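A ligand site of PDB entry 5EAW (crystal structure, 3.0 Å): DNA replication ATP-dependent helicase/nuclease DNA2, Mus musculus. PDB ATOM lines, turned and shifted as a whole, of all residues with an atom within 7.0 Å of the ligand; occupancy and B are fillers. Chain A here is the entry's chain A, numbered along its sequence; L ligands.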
ATOM      1  N   ARG A 136      18.448  -9.792  -8.627  1.00  0.00           N
ATOM      2  CA  ARG A 136      18.464  -8.511  -9.308  1.00  0.00           C
ATOM      3  C   ARG A 136      17.773  -8.548 -10.660  1.00  0.00           C
ATOM      4  O   ARG A 136      17.093  -7.598 -11.040  1.00  0.00           O
ATOM      5  CB  ARG A 136      19.896  -8.005  -9.426  1.00  0.00           C
ATOM      6  CG  ARG A 136      20.395  -7.321  -8.160  1.00  0.00           C
ATOM      7  CD  ARG A 136      20.490  -5.812  -8.318  1.00  0.00           C
ATOM      8  NE  ARG A 136      21.714  -5.306  -7.671  1.00  0.00           N
ATOM      9  CZ  ARG A 136      22.949  -5.377  -8.178  1.00  0.00           C
ATOM     10  NH1 ARG A 136      23.206  -5.920  -9.363  1.00  0.00           N
ATOM     11  NH2 ARG A 136      23.964  -4.877  -7.472  1.00  0.00           N
ATOM     12  N   CYS A 137      17.943  -9.639 -11.397  1.00  0.00           N
ATOM     13  CA  CYS A 137      17.370  -9.723 -12.736  1.00  0.00           C
ATOM     14  C   CYS A 137      17.231 -11.169 -13.215  1.00  0.00           C
ATOM     15  O   CYS A 137      18.216 -11.812 -13.548  1.00  0.00           O
ATOM     16  CB  CYS A 137      18.179  -8.878 -13.736  1.00  0.00           C
ATOM     17  SG  CYS A 137      17.599  -9.024 -15.432  1.00  0.00           S
ATOM     18  N   LEU A 138      15.986 -11.647 -13.266  1.00  0.00           N
ATOM     19  CA  LEU A 138      15.746 -13.030 -13.661  1.00  0.00           C
ATOM     20  C   LEU A 138      16.237 -13.311 -15.079  1.00  0.00           C
ATOM     21  O   LEU A 138      16.855 -14.361 -15.323  1.00  0.00           O
ATOM     22  CB  LEU A 138      14.271 -13.394 -13.493  1.00  0.00           C
ATOM     23  CG  LEU A 138      13.959 -14.878 -13.719  1.00  0.00           C
ATOM     24  CD1 LEU A 138      14.633 -15.775 -12.687  1.00  0.00           C
ATOM     25  CD2 LEU A 138      12.483 -15.120 -13.741  1.00  0.00           C
ATOM     26  N   ARG A 139      15.968 -12.381 -15.997  1.00  0.00           N
ATOM     27  CA  ARG A 139      16.431 -12.413 -17.392  1.00  0.00           C
ATOM     28  C   ARG A 139      17.965 -12.593 -17.486  1.00  0.00           C
ATOM     29  O   ARG A 139      18.447 -13.569 -18.063  1.00  0.00           O
ATOM     30  CB  ARG A 139      15.964 -11.144 -18.076  1.00  0.00           C
ATOM     31  CG  ARG A 139      16.237 -11.076 -19.570  1.00  0.00           C
ATOM     32  CD  ARG A 139      15.706  -9.752 -20.115  1.00  0.00           C
ATOM     33  NE  ARG A 139      15.943  -9.592 -21.557  1.00  0.00           N
ATOM     34  CZ  ARG A 139      15.144 -10.037 -22.528  1.00  0.00           C
ATOM     35  NH1 ARG A 139      14.021 -10.691 -22.233  1.00  0.00           N
ATOM     36  NH2 ARG A 139      15.481  -9.830 -23.788  1.00  0.00           N
ATOM     37  N   ARG A 140      18.711 -11.675 -16.874  1.00  0.00           N
ATOM     38  CA  ARG A 140      20.164 -11.798 -16.741  1.00  0.00           C
ATOM     39  C   ARG A 140      20.632 -13.228 -16.341  1.00  0.00           C
ATOM     40  O   ARG A 140      21.608 -13.740 -16.925  1.00  0.00           O
ATOM     41  CB  ARG A 140      20.701 -10.742 -15.767  1.00  0.00           C
ATOM     42  CG  ARG A 140      22.186 -10.449 -15.901  1.00  0.00           C
ATOM     43  CD  ARG A 140      22.961 -10.892 -14.672  1.00  0.00           C
ATOM     44  NE  ARG A 140      23.137  -9.796 -13.717  1.00  0.00           N
ATOM     45  CZ  ARG A 140      22.579  -9.721 -12.504  1.00  0.00           C
ATOM     46  NH1 ARG A 140      21.782 -10.696 -12.066  1.00  0.00           N
ATOM     47  NH2 ARG A 140      22.811  -8.664 -11.728  1.00  0.00           N
ATOM     48  N   ALA A 141      19.920 -13.851 -15.395  1.00  0.00           N
ATOM     49  CA  ALA A 141      20.222 -15.218 -14.929  1.00  0.00           C
ATOM     50  C   ALA A 141      19.986 -16.265 -16.015  1.00  0.00           C
ATOM     51  O   ALA A 141      20.850 -17.118 -16.268  1.00  0.00           O
ATOM     52  CB  ALA A 141      19.441 -15.541 -13.670  1.00  0.00           C
ATOM     53  N   LEU A 143      19.810 -15.830 -19.221  1.00  0.00           N
ATOM     54  CA  LEU A 143      20.707 -15.528 -20.309  1.00  0.00           C
ATOM     55  C   LEU A 143      22.064 -16.031 -19.955  1.00  0.00           C
ATOM     56  O   LEU A 143      22.730 -16.599 -20.801  1.00  0.00           O
ATOM     57  CB  LEU A 143      20.767 -14.036 -20.578  1.00  0.00           C
ATOM     58  CG  LEU A 143      19.717 -13.438 -21.483  1.00  0.00           C
ATOM     59  CD1 LEU A 143      19.737 -11.922 -21.360  1.00  0.00           C
ATOM     60  CD2 LEU A 143      19.891 -13.906 -22.923  1.00  0.00           C
ATOM     61  N   PRO A 385      11.991 -13.899 -19.307  1.00  0.00           N
ATOM     62  CA  PRO A 385      11.777 -12.889 -18.275  1.00  0.00           C
ATOM     63  C   PRO A 385      12.014 -11.465 -18.809  1.00  0.00           C
ATOM     64  O   PRO A 385      12.960 -11.239 -19.553  1.00  0.00           O
ATOM     65  CB  PRO A 385      12.782 -13.279 -17.204  1.00  0.00           C
ATOM     66  CG  PRO A 385      13.017 -14.752 -17.407  1.00  0.00           C
ATOM     67  CD  PRO A 385      12.337 -15.186 -18.672  1.00  0.00           C
ATOM     68  N   GLN A 386      11.127 -10.529 -18.471  1.00  0.00           N
ATOM     69  CA  GLN A 386      11.180  -9.220 -19.125  1.00  0.00           C
ATOM     70  C   GLN A 386      12.344  -8.346 -18.687  1.00  0.00           C
ATOM     71  O   GLN A 386      13.007  -8.632 -17.699  1.00  0.00           O
ATOM     72  CB  GLN A 386       9.825  -8.493 -19.055  1.00  0.00           C
ATOM     73  CG  GLN A 386       8.945  -8.781 -17.856  1.00  0.00           C
ATOM     74  CD  GLN A 386       7.927  -7.673 -17.675  1.00  0.00           C
ATOM     75  OE1 GLN A 386       7.341  -7.188 -18.655  1.00  0.00           O
ATOM     76  NE2 GLN A 386       7.723  -7.253 -16.426  1.00  0.00           N
ATOM     77  N   ILE A 387      12.608  -7.297 -19.462  1.00  0.00           N
ATOM     78  CA  ILE A 387      13.711  -6.371 -19.169  1.00  0.00           C
ATOM     79  C   ILE A 387      13.328  -5.474 -18.011  1.00  0.00           C
ATOM     80  O   ILE A 387      12.265  -4.843 -18.006  1.00  0.00           O
ATOM     81  CB  ILE A 387      14.106  -5.547 -20.410  1.00  0.00           C
ATOM     82  CG1 ILE A 387      14.527  -6.465 -21.560  1.00  0.00           C
ATOM     83  CG2 ILE A 387      15.211  -4.547 -20.071  1.00  0.00           C
ATOM     84  CD1 ILE A 387      14.405  -5.862 -22.940  1.00  0.00           C
ATOM     85  N   ILE A 388      14.224  -5.432 -17.037  1.00  0.00           N
ATOM     86  CA  ILE A 388      14.032  -4.685 -15.799  1.00  0.00           C
ATOM     87  C   ILE A 388      13.991  -3.173 -16.031  1.00  0.00           C
ATOM     88  O   ILE A 388      14.385  -2.697 -17.092  1.00  0.00           O
ATOM     89  CB  ILE A 388      15.104  -5.055 -14.718  1.00  0.00           C
ATOM     90  CG1 ILE A 388      16.526  -4.712 -15.201  1.00  0.00           C
ATOM     91  CG2 ILE A 388      14.958  -6.508 -14.276  1.00  0.00           C
ATOM     92  CD1 ILE A 388      17.576  -4.637 -14.117  1.00  0.00           C
ATOM     93  N   GLU A 389      13.494  -2.429 -15.027  1.00  0.00           N
ATOM     94  CA  GLU A 389      13.460  -0.955 -15.043  1.00  0.00           C
ATOM     95  C   GLU A 389      14.620  -0.354 -14.247  1.00  0.00           C
ATOM     96  O   GLU A 389      14.838   0.869 -14.275  1.00  0.00           O
ATOM     97  CB  GLU A 389      12.119  -0.460 -14.491  1.00  0.00           C
ATOM     98  CG  GLU A 389      11.596   0.755 -15.229  1.00  0.00           C
ATOM     99  CD  GLU A 389      10.101   0.669 -15.468  1.00  0.00           C
ATOM    100  OE1 GLU A 389       9.636  -0.294 -16.118  1.00  0.00           O
ATOM    101  OE2 GLU A 389       9.395   1.572 -15.000  1.00  0.00           O
ATOM    102  N   GLU A 390      15.366  -1.212 -13.565  1.00  0.00           N
ATOM    103  CA  GLU A 390      16.487  -0.829 -12.732  1.00  0.00           C
ATOM    104  C   GLU A 390      17.720  -0.496 -13.579  1.00  0.00           C
ATOM    105  O   GLU A 390      18.700  -1.243 -13.608  1.00  0.00           O
ATOM    106  CB  GLU A 390      16.764  -1.928 -11.686  1.00  0.00           C
ATOM    107  CG  GLU A 390      17.501  -1.481 -10.428  1.00  0.00           C
ATOM    108  CD  GLU A 390      16.739  -0.447  -9.599  1.00  0.00           C
ATOM    109  OE1 GLU A 390      17.418   0.404  -8.978  1.00  0.00           O
ATOM    110  OE2 GLU A 390      15.484  -0.477  -9.566  1.00  0.00           O
ATOM    111  N   THR A 393      21.373  -1.392 -12.611  1.00  0.00           N
ATOM    112  CA  THR A 393      21.748  -2.822 -12.738  1.00  0.00           C
ATOM    113  C   THR A 393      22.201  -3.121 -14.173  1.00  0.00           C
ATOM    114  O   THR A 393      23.308  -3.623 -14.390  1.00  0.00           O
ATOM    115  CB  THR A 393      20.622  -3.823 -12.328  1.00  0.00           C
ATOM    116  OG1 THR A 393      20.032  -3.432 -11.091  1.00  0.00           O
ATOM    117  CG2 THR A 393      21.180  -5.243 -12.162  1.00  0.00           C
ATOM    118  N   CYS A 394      21.327  -2.780 -15.123  1.00  0.00           N
ATOM    119  CA  CYS A 394      21.601  -2.883 -16.563  1.00  0.00           C
ATOM    120  C   CYS A 394      22.999  -2.371 -16.968  1.00  0.00           C
ATOM    121  O   CYS A 394      23.770  -3.122 -17.556  1.00  0.00           O
ATOM    122  CB  CYS A 394      20.520  -2.146 -17.360  1.00  0.00           C
ATOM    123  SG  CYS A 394      18.863  -2.871 -17.291  1.00  0.00           S
ATOM    124  N   LYS A 395      23.317  -1.122 -16.587  1.00  0.00           N
ATOM    125  CA  LYS A 395      24.513  -0.419 -17.056  1.00  0.00           C
ATOM    126  C   LYS A 395      25.734  -1.314 -17.246  1.00  0.00           C
ATOM    127  O   LYS A 395      26.321  -1.340 -18.332  1.00  0.00           O
ATOM    128  CB  LYS A 395      24.841   0.791 -16.138  1.00  0.00           C
ATOM    129  CG  LYS A 395      24.107   2.088 -16.478  1.00  0.00           C
ATOM    130  CD  LYS A 395      24.710   2.808 -17.694  1.00  0.00           C
ATOM    131  CE  LYS A 395      24.482   4.303 -17.646  1.00  0.00           C
ATOM    132  NZ  LYS A 395      25.258   5.006 -18.707  1.00  0.00           N
ATOM    133  N   TYR A 396      26.062  -2.079 -16.204  1.00  0.00           N
ATOM    134  CA  TYR A 396      27.194  -2.994 -16.221  1.00  0.00           C
ATOM    135  C   TYR A 396      26.692  -4.433 -16.254  1.00  0.00           C
ATOM    136  O   TYR A 396      26.681  -5.110 -15.227  1.00  0.00           O
ATOM    137  CB  TYR A 396      28.074  -2.772 -14.986  1.00  0.00           C
ATOM    138  CG  TYR A 396      28.770  -1.423 -14.924  1.00  0.00           C
ATOM    139  CD1 TYR A 396      29.934  -1.169 -15.679  1.00  0.00           C
ATOM    140  CD2 TYR A 396      28.284  -0.397 -14.081  1.00  0.00           C
ATOM    141  CE1 TYR A 396      30.577   0.059 -15.622  1.00  0.00           C
ATOM    142  CE2 TYR A 396      28.933   0.834 -14.016  1.00  0.00           C
ATOM    143  CZ  TYR A 396      30.072   1.056 -14.791  1.00  0.00           C
ATOM    144  OH  TYR A 396      30.712   2.268 -14.738  1.00  0.00           O
ATOM    145  N   CYS A 397      26.277  -4.924 -17.412  1.00  0.00           N
ATOM    146  CA  CYS A 397      25.709  -6.273 -17.487  1.00  0.00           C
ATOM    147  C   CYS A 397      26.536  -7.356 -18.213  1.00  0.00           C
ATOM    148  O   CYS A 397      26.654  -8.478 -17.689  1.00  0.00           O
ATOM    149  CB  CYS A 397      24.283  -6.249 -18.037  1.00  0.00           C
ATOM    150  SG  CYS A 397      23.395  -7.784 -17.683  1.00  0.00           S
ATOM    151  N   SER A 398      27.082  -7.013 -19.392  1.00  0.00           N
ATOM    152  CA  SER A 398      27.787  -7.944 -20.325  1.00  0.00           C
ATOM    153  C   SER A 398      26.815  -8.878 -21.055  1.00  0.00           C
ATOM    154  O   SER A 398      27.048  -9.289 -22.186  1.00  0.00           O
ATOM    155  CB  SER A 398      28.890  -8.768 -19.650  1.00  0.00           C
ATOM    156  OG  SER A 398      28.331  -9.879 -18.964  1.00  0.00           O
ATOM    157  N   GLN A 399      25.732  -9.211 -20.351  1.00  0.00           N
ATOM    158  CA  GLN A 399      24.640  -9.976 -20.883  1.00  0.00           C
ATOM    159  C   GLN A 399      23.691  -9.055 -21.680  1.00  0.00           C
ATOM    160  O   GLN A 399      22.923  -9.543 -22.488  1.00  0.00           O
ATOM    161  CB  GLN A 399      23.945 -10.671 -19.715  1.00  0.00           C
ATOM    162  CG  GLN A 399      23.429 -12.072 -19.986  1.00  0.00           C
ATOM    163  CD  GLN A 399      24.473 -13.064 -20.489  1.00  0.00           C
ATOM    164  OE1 GLN A 399      24.578 -13.312 -21.686  1.00  0.00           O
ATOM    165  NE2 GLN A 399      25.247 -13.647 -19.577  1.00  0.00           N
ATOM    166  N   ILE A 400      23.781  -7.736 -21.476  1.00  0.00           N
ATOM    167  CA  ILE A 400      23.124  -6.694 -22.308  1.00  0.00           C
ATOM    168  C   ILE A 400      23.202  -6.948 -23.832  1.00  0.00           C
ATOM    169  O   ILE A 400      22.226  -6.696 -24.559  1.00  0.00           O
ATOM    170  CB  ILE A 400      23.654  -5.260 -21.958  1.00  0.00           C
ATOM    171  CG1 ILE A 400      23.355  -4.214 -23.044  1.00  0.00           C
ATOM    172  CG2 ILE A 400      25.157  -5.275 -21.735  1.00  0.00           C
ATOM    173  CD1 ILE A 400      22.030  -3.494 -22.890  1.00  0.00           C
ATOM    174  N   GLY A 401      24.358  -7.448 -24.291  1.00  0.00           N
ATOM    175  CA  GLY A 401      24.552  -7.850 -25.695  1.00  0.00           C
ATOM    176  C   GLY A 401      23.516  -8.844 -26.174  1.00  0.00           C
ATOM    177  O   GLY A 401      22.786  -8.574 -27.133  1.00  0.00           O
ATOM    178  N   ASN A 402      23.427  -9.984 -25.486  1.00  0.00           N
ATOM    179  CA  ASN A 402      22.404 -11.014 -25.741  1.00  0.00           C
ATOM    180  C   ASN A 402      20.986 -10.607 -25.395  1.00  0.00           C
ATOM    181  O   ASN A 402      20.048 -11.071 -26.016  1.00  0.00           O
ATOM    182  CB  ASN A 402      22.727 -12.298 -24.988  1.00  0.00           C
ATOM    183  CG  ASN A 402      24.024 -12.923 -25.431  1.00  0.00           C
ATOM    184  OD1 ASN A 402      24.314 -13.080 -26.615  1.00  0.00           O
ATOM    185  ND2 ASN A 402      24.815 -13.292 -24.462  1.00  0.00           N
ATOM    186  N   CYS A 403      20.842  -9.765 -24.384  1.00  0.00           N
ATOM    187  CA  CYS A 403      19.545  -9.261 -23.969  1.00  0.00           C
ATOM    188  C   CYS A 403      18.940  -8.405 -25.072  1.00  0.00           C
ATOM    189  O   CYS A 403      17.781  -8.651 -25.458  1.00  0.00           O
ATOM    190  CB  CYS A 403      19.689  -8.458 -22.682  1.00  0.00           C
ATOM    191  SG  CYS A 403      18.149  -7.709 -22.105  1.00  0.00           S
ATOM    192  N   ALA A 404      19.720  -7.441 -25.585  1.00  0.00           N
ATOM    193  CA  ALA A 404      19.288  -6.564 -26.676  1.00  0.00           C
ATOM    194  C   ALA A 404      19.004  -7.416 -27.911  1.00  0.00           C
ATOM    195  O   ALA A 404      17.936  -7.289 -28.561  1.00  0.00           O
ATOM    196  CB  ALA A 404      20.323  -5.497 -26.972  1.00  0.00           C
ATOM    197  N   MET A 423      16.234   2.062 -22.009  1.00  0.00           N
ATOM    198  CA  MET A 423      16.722   0.762 -22.473  1.00  0.00           C
ATOM    199  C   MET A 423      16.378   0.529 -23.953  1.00  0.00           C
ATOM    200  O   MET A 423      17.203   0.000 -24.694  1.00  0.00           O
ATOM    201  CB  MET A 423      16.153  -0.346 -21.575  1.00  0.00           C
ATOM    202  CG  MET A 423      16.759  -1.719 -21.771  1.00  0.00           C
ATOM    203  SD  MET A 423      18.504  -1.861 -21.321  1.00  0.00           S
ATOM    204  CE  MET A 423      18.713  -3.636 -21.398  1.00  0.00           C
HETATM  205 FE1  LIG L   1      18.515  -8.036 -17.144  1.00  0.00          FE
HETATM  206 FE2  LIG L   1      19.043  -7.155 -20.021  1.00  0.00          FE
HETATM  207 FE3  LIG L   1      21.262  -7.701 -18.145  1.00  0.00          FE
HETATM  208 FE4  LIG L   1      19.564  -5.354 -17.803  1.00  0.00          FE
HETATM  209  S1  LIG L   1      20.755  -6.062 -19.439  1.00  0.00           S
HETATM  210  S2  LIG L   1      20.172  -6.922 -16.468  1.00  0.00           S
HETATM  211  S3  LIG L   1      17.841  -6.453 -18.401  1.00  0.00           S
HETATM  212  S4  LIG L   1      19.580  -8.843 -18.805  1.00  0.00           S
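Residues that only touch the ligand: Ile 387, Ile 388, Ile 400 and Met 423. Hydrophobic or aromatic side chains within 4 Å of the ligand: Ile 387, Ile 388, Ile 400 and Met 423. Along chain A the residues within 4 Å of the ligand span positions 137 to 423. The nearest printed residue that does not touch the ligand is Leu 143 (4.004 Å).
The side-chain sulfur of Cys 137 binds an iron atom (FE1) of the ligand (2.2 Å). An iron atom (FE3) of the ligand is bound by the side-chain sulfur (SG) of Cys 397, 2.2 Å away. FE2 of the ligand is bound by SG of Cys 403 (2.3 Å). An iron atom (FE4) of the ligand is bound by the side-chain sulfur of Cys 394 (2.6 Å). The backbone NH (N) of Arg 140 lies close to a sulfur (S4) of the ligand.
The side-chain sulfur (SG) of Cys 137 lies close to the backbone NH (N) of Arg 140, at 3.2 Å. The side-chain sulfur (SG) of Cys 137 lies close to the backbone NH (N) of Arg 139, 3.8 Å away. O of Cys 403 is in hydrogen-bond range of NH2 of Arg 139, 3.1 Å away.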
